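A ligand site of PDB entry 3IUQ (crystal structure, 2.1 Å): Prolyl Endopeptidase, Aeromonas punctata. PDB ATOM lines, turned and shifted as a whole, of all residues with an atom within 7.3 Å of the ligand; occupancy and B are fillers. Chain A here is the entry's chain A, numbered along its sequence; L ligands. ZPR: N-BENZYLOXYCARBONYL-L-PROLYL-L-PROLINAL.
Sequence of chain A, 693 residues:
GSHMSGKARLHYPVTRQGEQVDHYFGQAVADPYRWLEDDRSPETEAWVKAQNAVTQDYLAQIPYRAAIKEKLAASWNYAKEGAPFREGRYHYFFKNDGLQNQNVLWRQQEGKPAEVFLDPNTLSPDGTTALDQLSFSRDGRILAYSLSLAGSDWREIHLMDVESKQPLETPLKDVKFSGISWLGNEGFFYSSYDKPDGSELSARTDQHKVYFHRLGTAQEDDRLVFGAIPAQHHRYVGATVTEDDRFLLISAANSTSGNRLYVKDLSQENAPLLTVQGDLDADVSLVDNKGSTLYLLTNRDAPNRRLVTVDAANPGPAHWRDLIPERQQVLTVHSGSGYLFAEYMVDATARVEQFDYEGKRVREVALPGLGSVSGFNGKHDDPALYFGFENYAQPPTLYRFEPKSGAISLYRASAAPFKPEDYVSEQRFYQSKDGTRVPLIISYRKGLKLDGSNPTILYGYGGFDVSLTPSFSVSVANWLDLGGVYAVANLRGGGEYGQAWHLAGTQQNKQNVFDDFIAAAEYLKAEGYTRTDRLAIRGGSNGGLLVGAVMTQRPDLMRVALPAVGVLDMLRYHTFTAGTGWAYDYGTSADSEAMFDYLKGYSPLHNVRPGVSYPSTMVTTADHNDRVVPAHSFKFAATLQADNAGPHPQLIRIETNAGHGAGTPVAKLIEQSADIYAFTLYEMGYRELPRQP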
ATOM      1  N   ASP A 153      -7.463  31.073 -14.252  1.00  0.00           N
ATOM      2  CA  ASP A 153      -8.068  30.696 -15.519  1.00  0.00           C
ATOM      3  C   ASP A 153      -9.497  31.238 -15.642  1.00  0.00           C
ATOM      4  O   ASP A 153     -10.125  31.096 -16.687  1.00  0.00           O
ATOM      5  CB  ASP A 153      -8.054  29.163 -15.667  1.00  0.00           C
ATOM      6  CG  ASP A 153      -6.687  28.626 -16.108  1.00  0.00           C
ATOM      7  OD1 ASP A 153      -6.356  27.473 -15.748  1.00  0.00           O
ATOM      8  OD2 ASP A 153      -5.946  29.336 -16.824  1.00  0.00           O
ATOM      9  N   PHE A 177     -12.071  29.019 -19.855  1.00  0.00           N
ATOM     10  CA  PHE A 177     -11.643  28.267 -21.044  1.00  0.00           C
ATOM     11  C   PHE A 177     -12.675  28.522 -22.128  1.00  0.00           C
ATOM     12  O   PHE A 177     -13.170  27.590 -22.777  1.00  0.00           O
ATOM     13  CB  PHE A 177     -11.568  26.772 -20.748  1.00  0.00           C
ATOM     14  CG  PHE A 177     -10.682  26.424 -19.591  1.00  0.00           C
ATOM     15  CD1 PHE A 177      -9.408  26.985 -19.459  1.00  0.00           C
ATOM     16  CD2 PHE A 177     -11.095  25.502 -18.633  1.00  0.00           C
ATOM     17  CE1 PHE A 177      -8.563  26.639 -18.416  1.00  0.00           C
ATOM     18  CE2 PHE A 177     -10.262  25.134 -17.574  1.00  0.00           C
ATOM     19  CZ  PHE A 177      -8.989  25.707 -17.464  1.00  0.00           C
ATOM     20  N   TYR A 236     -14.360  20.084 -21.612  1.00  0.00           N
ATOM     21  CA  TYR A 236     -14.086  21.311 -22.377  1.00  0.00           C
ATOM     22  C   TYR A 236     -14.965  21.428 -23.621  1.00  0.00           C
ATOM     23  O   TYR A 236     -14.993  20.519 -24.440  1.00  0.00           O
ATOM     24  CB  TYR A 236     -12.618  21.346 -22.850  1.00  0.00           C
ATOM     25  CG  TYR A 236     -11.571  21.182 -21.765  1.00  0.00           C
ATOM     26  CD1 TYR A 236     -11.427  22.131 -20.753  1.00  0.00           C
ATOM     27  CD2 TYR A 236     -10.724  20.073 -21.751  1.00  0.00           C
ATOM     28  CE1 TYR A 236     -10.465  21.976 -19.757  1.00  0.00           C
ATOM     29  CE2 TYR A 236      -9.757  19.917 -20.747  1.00  0.00           C
ATOM     30  CZ  TYR A 236      -9.637  20.869 -19.756  1.00  0.00           C
ATOM     31  OH  TYR A 236      -8.706  20.702 -18.755  1.00  0.00           O
ATOM     32  N   SER A 255     -10.010  15.875 -22.879  1.00  0.00           N
ATOM     33  CA  SER A 255      -8.578  15.974 -22.644  1.00  0.00           C
ATOM     34  C   SER A 255      -7.948  16.963 -23.614  1.00  0.00           C
ATOM     35  O   SER A 255      -8.637  17.576 -24.416  1.00  0.00           O
ATOM     36  CB  SER A 255      -7.933  14.590 -22.810  1.00  0.00           C
ATOM     37  OG  SER A 255      -6.625  14.578 -22.262  1.00  0.00           O
ATOM     38  N   THR A 256      -6.632  17.109 -23.538  1.00  0.00           N
ATOM     39  CA  THR A 256      -5.923  18.057 -24.396  1.00  0.00           C
ATOM     40  C   THR A 256      -5.780  17.664 -25.870  1.00  0.00           C
ATOM     41  O   THR A 256      -5.365  18.477 -26.679  1.00  0.00           O
ATOM     42  CB  THR A 256      -4.543  18.374 -23.807  1.00  0.00           C
ATOM     43  OG1 THR A 256      -3.887  17.150 -23.455  1.00  0.00           O
ATOM     44  CG2 THR A 256      -4.699  19.238 -22.564  1.00  0.00           C
ATOM     45  N   TYR A 461      10.550  21.277 -24.022  1.00  0.00           N
ATOM     46  CA  TYR A 461       9.184  21.152 -23.524  1.00  0.00           C
ATOM     47  C   TYR A 461       8.860  19.673 -23.692  1.00  0.00           C
ATOM     48  O   TYR A 461       8.894  18.913 -22.729  1.00  0.00           O
ATOM     49  CB  TYR A 461       8.234  22.034 -24.358  1.00  0.00           C
ATOM     50  CG  TYR A 461       6.819  22.133 -23.808  1.00  0.00           C
ATOM     51  CD1 TYR A 461       6.550  22.895 -22.662  1.00  0.00           C
ATOM     52  CD2 TYR A 461       5.764  21.453 -24.412  1.00  0.00           C
ATOM     53  CE1 TYR A 461       5.243  22.968 -22.130  1.00  0.00           C
ATOM     54  CE2 TYR A 461       4.465  21.517 -23.886  1.00  0.00           C
ATOM     55  CZ  TYR A 461       4.214  22.271 -22.750  1.00  0.00           C
ATOM     56  OH  TYR A 461       2.932  22.330 -22.257  1.00  0.00           O
ATOM     57  N   GLY A 463       5.902  17.722 -25.278  1.00  0.00           N
ATOM     58  CA  GLY A 463       4.611  17.210 -24.898  1.00  0.00           C
ATOM     59  C   GLY A 463       3.430  17.992 -25.460  1.00  0.00           C
ATOM     60  O   GLY A 463       3.593  19.091 -26.014  1.00  0.00           O
ATOM     61  N   PHE A 464       2.258  17.378 -25.378  1.00  0.00           N
ATOM     62  CA  PHE A 464       1.004  18.000 -25.789  1.00  0.00           C
ATOM     63  C   PHE A 464       0.937  18.523 -27.221  1.00  0.00           C
ATOM     64  O   PHE A 464       0.222  19.475 -27.499  1.00  0.00           O
ATOM     65  CB  PHE A 464       0.695  19.120 -24.779  1.00  0.00           C
ATOM     66  CG  PHE A 464       0.563  18.614 -23.371  1.00  0.00           C
ATOM     67  CD1 PHE A 464      -0.667  18.209 -22.864  1.00  0.00           C
ATOM     68  CD2 PHE A 464       1.696  18.456 -22.564  1.00  0.00           C
ATOM     69  CE1 PHE A 464      -0.772  17.659 -21.580  1.00  0.00           C
ATOM     70  CE2 PHE A 464       1.614  17.896 -21.283  1.00  0.00           C
ATOM     71  CZ  PHE A 464       0.364  17.502 -20.787  1.00  0.00           C
ATOM     72  N   VAL A 466       2.815  20.287 -28.749  1.00  0.00           N
ATOM     73  CA  VAL A 466       3.291  21.670 -28.839  1.00  0.00           C
ATOM     74  C   VAL A 466       4.586  21.729 -29.639  1.00  0.00           C
ATOM     75  O   VAL A 466       5.509  20.967 -29.390  1.00  0.00           O
ATOM     76  CB  VAL A 466       3.541  22.272 -27.428  1.00  0.00           C
ATOM     77  CG1 VAL A 466       4.332  23.576 -27.544  1.00  0.00           C
ATOM     78  CG2 VAL A 466       2.186  22.528 -26.745  1.00  0.00           C
ATOM     79  N   GLY A 540       9.601  25.030 -18.741  1.00  0.00           N
ATOM     80  CA  GLY A 540       8.448  25.504 -17.989  1.00  0.00           C
ATOM     81  C   GLY A 540       7.203  24.639 -18.100  1.00  0.00           C
ATOM     82  O   GLY A 540       6.778  24.310 -19.222  1.00  0.00           O
ATOM     83  N   SER A 541       6.602  24.274 -16.953  1.00  0.00           N
ATOM     84  CA  SER A 541       5.381  23.449 -16.889  1.00  0.00           C
ATOM     85  C   SER A 541       5.604  21.974 -17.229  1.00  0.00           C
ATOM     86  O   SER A 541       5.997  21.176 -16.371  1.00  0.00           O
ATOM     87  CB  SER A 541       4.311  24.045 -17.800  1.00  0.00           C
ATOM     88  OG  SER A 541       3.843  25.282 -17.299  1.00  0.00           O
ATOM     89  N   ASN A 542       5.297  21.581 -18.460  1.00  0.00           N
ATOM     90  CA  ASN A 542       5.567  20.215 -18.862  1.00  0.00           C
ATOM     91  C   ASN A 542       7.083  20.204 -19.032  1.00  0.00           C
ATOM     92  O   ASN A 542       7.730  19.168 -18.909  1.00  0.00           O
ATOM     93  CB  ASN A 542       4.889  19.843 -20.179  1.00  0.00           C
ATOM     94  CG  ASN A 542       5.422  18.536 -20.759  1.00  0.00           C
ATOM     95  OD1 ASN A 542       6.135  18.534 -21.766  1.00  0.00           O
ATOM     96  ND2 ASN A 542       5.112  17.421 -20.100  1.00  0.00           N
ATOM     97  N   GLY A 543       7.623  21.390 -19.307  1.00  0.00           N
ATOM     98  CA  GLY A 543       9.058  21.554 -19.447  1.00  0.00           C
ATOM     99  C   GLY A 543       9.690  21.544 -18.051  1.00  0.00           C
ATOM    100  O   GLY A 543      10.884  21.283 -17.892  1.00  0.00           O
ATOM    101  N   LEU A 545       8.557  19.551 -15.804  1.00  0.00           N
ATOM    102  CA  LEU A 545       8.583  18.130 -15.541  1.00  0.00           C
ATOM    103  C   LEU A 545       9.837  17.558 -16.211  1.00  0.00           C
ATOM    104  O   LEU A 545      10.541  16.729 -15.625  1.00  0.00           O
ATOM    105  CB  LEU A 545       7.340  17.463 -16.129  1.00  0.00           C
ATOM    106  CG  LEU A 545       7.424  15.956 -16.394  1.00  0.00           C
ATOM    107  CD1 LEU A 545       7.729  15.232 -15.085  1.00  0.00           C
ATOM    108  CD2 LEU A 545       6.133  15.464 -17.017  1.00  0.00           C
ATOM    109  N   VAL A 565       7.442  26.348 -12.741  1.00  0.00           N
ATOM    110  CA  VAL A 565       6.028  25.962 -12.682  1.00  0.00           C
ATOM    111  C   VAL A 565       5.810  24.538 -13.205  1.00  0.00           C
ATOM    112  O   VAL A 565       4.857  24.268 -13.928  1.00  0.00           O
ATOM    113  CB  VAL A 565       5.156  26.935 -13.504  1.00  0.00           C
ATOM    114  CG1 VAL A 565       3.686  26.718 -13.188  1.00  0.00           C
ATOM    115  CG2 VAL A 565       5.551  28.369 -13.196  1.00  0.00           C
ATOM    116  N   GLY A 566       6.700  23.637 -12.813  1.00  0.00           N
ATOM    117  CA  GLY A 566       6.581  22.271 -13.294  1.00  0.00           C
ATOM    118  C   GLY A 566       5.627  21.335 -12.585  1.00  0.00           C
ATOM    119  O   GLY A 566       5.242  21.539 -11.431  1.00  0.00           O
ATOM    120  N   VAL A 567       5.244  20.296 -13.320  1.00  0.00           N
ATOM    121  CA  VAL A 567       4.379  19.244 -12.801  1.00  0.00           C
ATOM    122  C   VAL A 567       5.455  18.293 -12.289  1.00  0.00           C
ATOM    123  O   VAL A 567       6.193  17.702 -13.083  1.00  0.00           O
ATOM    124  CB  VAL A 567       3.590  18.554 -13.938  1.00  0.00           C
ATOM    125  CG1 VAL A 567       2.610  17.551 -13.348  1.00  0.00           C
ATOM    126  CG2 VAL A 567       2.845  19.602 -14.767  1.00  0.00           C
ATOM    127  N   ALA A 578      -6.478  21.779 -13.254  1.00  0.00           N
ATOM    128  CA  ALA A 578      -6.666  21.481 -14.669  1.00  0.00           C
ATOM    129  C   ALA A 578      -5.963  20.185 -14.963  1.00  0.00           C
ATOM    130  O   ALA A 578      -5.964  19.748 -16.106  1.00  0.00           O
ATOM    131  CB  ALA A 578      -6.088  22.577 -15.529  1.00  0.00           C
ATOM    132  N   GLY A 579      -5.374  19.572 -13.930  1.00  0.00           N
ATOM    133  CA  GLY A 579      -4.661  18.301 -14.100  1.00  0.00           C
ATOM    134  C   GLY A 579      -5.516  17.173 -14.623  1.00  0.00           C
ATOM    135  O   GLY A 579      -5.051  16.234 -15.264  1.00  0.00           O
ATOM    136  N   GLY A 581      -7.376  17.205 -16.958  1.00  0.00           N
ATOM    137  CA  GLY A 581      -7.443  17.266 -18.404  1.00  0.00           C
ATOM    138  C   GLY A 581      -6.185  16.856 -19.163  1.00  0.00           C
ATOM    139  O   GLY A 581      -6.167  16.973 -20.386  1.00  0.00           O
ATOM    140  N   TRP A 582      -5.155  16.366 -18.472  1.00  0.00           N
ATOM    141  CA  TRP A 582      -3.917  15.977 -19.160  1.00  0.00           C
ATOM    142  C   TRP A 582      -3.647  14.476 -19.276  1.00  0.00           C
ATOM    143  O   TRP A 582      -2.531  14.064 -19.631  1.00  0.00           O
ATOM    144  CB  TRP A 582      -2.696  16.633 -18.491  1.00  0.00           C
ATOM    145  CG  TRP A 582      -2.835  18.101 -18.165  1.00  0.00           C
ATOM    146  CD1 TRP A 582      -3.456  19.062 -18.911  1.00  0.00           C
ATOM    147  CD2 TRP A 582      -2.316  18.771 -17.002  1.00  0.00           C
ATOM    148  NE1 TRP A 582      -3.371  20.279 -18.288  1.00  0.00           N
ATOM    149  CE2 TRP A 582      -2.678  20.125 -17.115  1.00  0.00           C
ATOM    150  CE3 TRP A 582      -1.595  18.343 -15.887  1.00  0.00           C
ATOM    151  CZ2 TRP A 582      -2.329  21.073 -16.128  1.00  0.00           C
ATOM    152  CZ3 TRP A 582      -1.251  19.282 -14.909  1.00  0.00           C
ATOM    153  CH2 TRP A 582      -1.613  20.629 -15.045  1.00  0.00           C
ATOM    154  N   ASP A 585      -1.851  12.806 -22.427  1.00  0.00           N
ATOM    155  CA  ASP A 585      -0.391  12.870 -22.477  1.00  0.00           C
ATOM    156  C   ASP A 585       0.331  12.121 -21.372  1.00  0.00           C
ATOM    157  O   ASP A 585       1.412  11.592 -21.604  1.00  0.00           O
ATOM    158  CB  ASP A 585       0.076  14.320 -22.450  1.00  0.00           C
ATOM    159  CG  ASP A 585       0.432  14.837 -23.823  1.00  0.00           C
ATOM    160  OD1 ASP A 585       1.647  14.877 -24.151  1.00  0.00           O
ATOM    161  OD2 ASP A 585      -0.497  15.194 -24.562  1.00  0.00           O
ATOM    162  N   TYR A 586      -0.246  12.082 -20.170  1.00  0.00           N
ATOM    163  CA  TYR A 586       0.442  11.441 -19.046  1.00  0.00           C
ATOM    164  C   TYR A 586      -0.119  10.133 -18.519  1.00  0.00           C
ATOM    165  O   TYR A 586       0.620   9.318 -17.950  1.00  0.00           O
ATOM    166  CB  TYR A 586       0.489  12.372 -17.819  1.00  0.00           C
ATOM    167  CG  TYR A 586       1.192  13.700 -17.986  1.00  0.00           C
ATOM    168  CD1 TYR A 586       2.333  13.823 -18.761  1.00  0.00           C
ATOM    169  CD2 TYR A 586       0.732  14.835 -17.304  1.00  0.00           C
ATOM    170  CE1 TYR A 586       3.011  15.052 -18.866  1.00  0.00           C
ATOM    171  CE2 TYR A 586       1.401  16.064 -17.404  1.00  0.00           C
ATOM    172  CZ  TYR A 586       2.538  16.157 -18.192  1.00  0.00           C
ATOM    173  OH  TYR A 586       3.189  17.367 -18.307  1.00  0.00           O
ATOM    174  N   ARG A 627      -3.322  26.940 -13.267  1.00  0.00           N
ATOM    175  CA  ARG A 627      -3.000  25.850 -14.189  1.00  0.00           C
ATOM    176  C   ARG A 627      -2.176  24.725 -13.541  1.00  0.00           C
ATOM    177  O   ARG A 627      -2.595  23.563 -13.518  1.00  0.00           O
ATOM    178  CB  ARG A 627      -2.270  26.391 -15.426  1.00  0.00           C
ATOM    179  CG  ARG A 627      -2.150  25.403 -16.569  1.00  0.00           C
ATOM    180  CD  ARG A 627      -3.517  24.896 -17.000  1.00  0.00           C
ATOM    181  NE  ARG A 627      -4.358  25.990 -17.480  1.00  0.00           N
ATOM    182  CZ  ARG A 627      -4.170  26.618 -18.642  1.00  0.00           C
ATOM    183  NH1 ARG A 627      -3.180  26.246 -19.441  1.00  0.00           N
ATOM    184  NH2 ARG A 627      -4.975  27.607 -18.992  1.00  0.00           N
ATOM    185  N   VAL A 628      -1.011  25.076 -13.023  1.00  0.00           N
ATOM    186  CA  VAL A 628      -0.121  24.114 -12.372  1.00  0.00           C
ATOM    187  C   VAL A 628       0.042  24.567 -10.915  1.00  0.00           C
ATOM    188  O   VAL A 628       0.681  25.580 -10.651  1.00  0.00           O
ATOM    189  CB  VAL A 628       1.267  24.091 -13.059  1.00  0.00           C
ATOM    190  CG1 VAL A 628       2.196  23.122 -12.339  1.00  0.00           C
ATOM    191  CG2 VAL A 628       1.118  23.711 -14.540  1.00  0.00           C
HETATM  192  O17 ZPR L   1      -5.542  23.424 -21.526  1.00  0.00           O
HETATM  193  C15 ZPR L   1      -4.425  22.821 -21.047  1.00  0.00           C
HETATM  194  O16 ZPR L   1      -4.416  22.401 -19.907  1.00  0.00           O
HETATM  195  N14 ZPR L   1      -3.322  22.704 -21.849  1.00  0.00           N
HETATM  196  C10 ZPR L   1      -2.009  22.080 -21.495  1.00  0.00           C
HETATM  197  C8  ZPR L   1      -1.343  22.781 -20.309  1.00  0.00           C
HETATM  198  O9  ZPR L   1      -1.601  23.946 -20.085  1.00  0.00           O
HETATM  199  C11 ZPR L   1      -1.110  22.194 -22.745  1.00  0.00           C
HETATM  200  C12 ZPR L   1      -1.731  23.371 -23.538  1.00  0.00           C
HETATM  201  C13 ZPR L   1      -3.244  23.187 -23.252  1.00  0.00           C
HETATM  202  C4  ZPR L   1       0.898  21.577 -17.529  1.00  0.00           C
HETATM  203  C5  ZPR L   1       0.991  20.390 -18.528  1.00  0.00           C
HETATM  204  C1  ZPR L   1       1.267  23.771 -18.766  1.00  0.00           C
HETATM  205  O2  ZPR L   1       2.184  23.215 -19.728  1.00  0.00           O
HETATM  206  N7  ZPR L   1      -0.450  22.122 -19.500  1.00  0.00           N
HETATM  207  C6  ZPR L   1      -0.018  20.719 -19.640  1.00  0.00           C
HETATM  208  C3  ZPR L   1       0.250  22.735 -18.332  1.00  0.00           C
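The side-chain hydroxyl (OH) of Tyr 461 is in hydrogen-bond range of an oxygen (O2) of the ligand (2.8 Å). An oxygen (O9) of the ligand is in hydrogen-bond range of the guanidinium group of Arg 627 (2.9 Å). An oxygen (O16) of the ligand lies within hydrogen-bond range of the indole nitrogen of Trp 582 (2.9 Å).
O of Tyr 461 sits close to OD1 of Asn 542 (2.9 Å). The guanidinium group (NH2) of Arg 627 is in salt-bridge range of the side-chain carboxylate (OD2) of Asp 153, 2.9 Å away. The backbone carbonyl oxygen (O) of Ala 578 sits at hydrogen-bond distance from the indole nitrogen (NE1) of Trp 582 (3.4 Å). The backbone carbonyl oxygen (O) of Ser 541 lies within hydrogen-bond range of the backbone NH (N) of Val 567 (3.3 Å). O of Val 565 sits close to N of Ser 541, 3.5 Å away. N of Phe 464 is in hydrogen-bond range of OD1 of Asp 585 (2.9 Å). The side-chain amide nitrogen of Asn 542 is in hydrogen-bond range of the side-chain hydroxyl of Tyr 586, at 2.6 Å. The backbone NH (N) of Thr 256 is in hydrogen-bond range of the backbone carbonyl oxygen (O) of Gly 581 (3.2 Å).
Residues that only touch the ligand: Thr 256, Phe 464, Ser 541, Asn 542, Val 567, Tyr 586 and Val 628.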
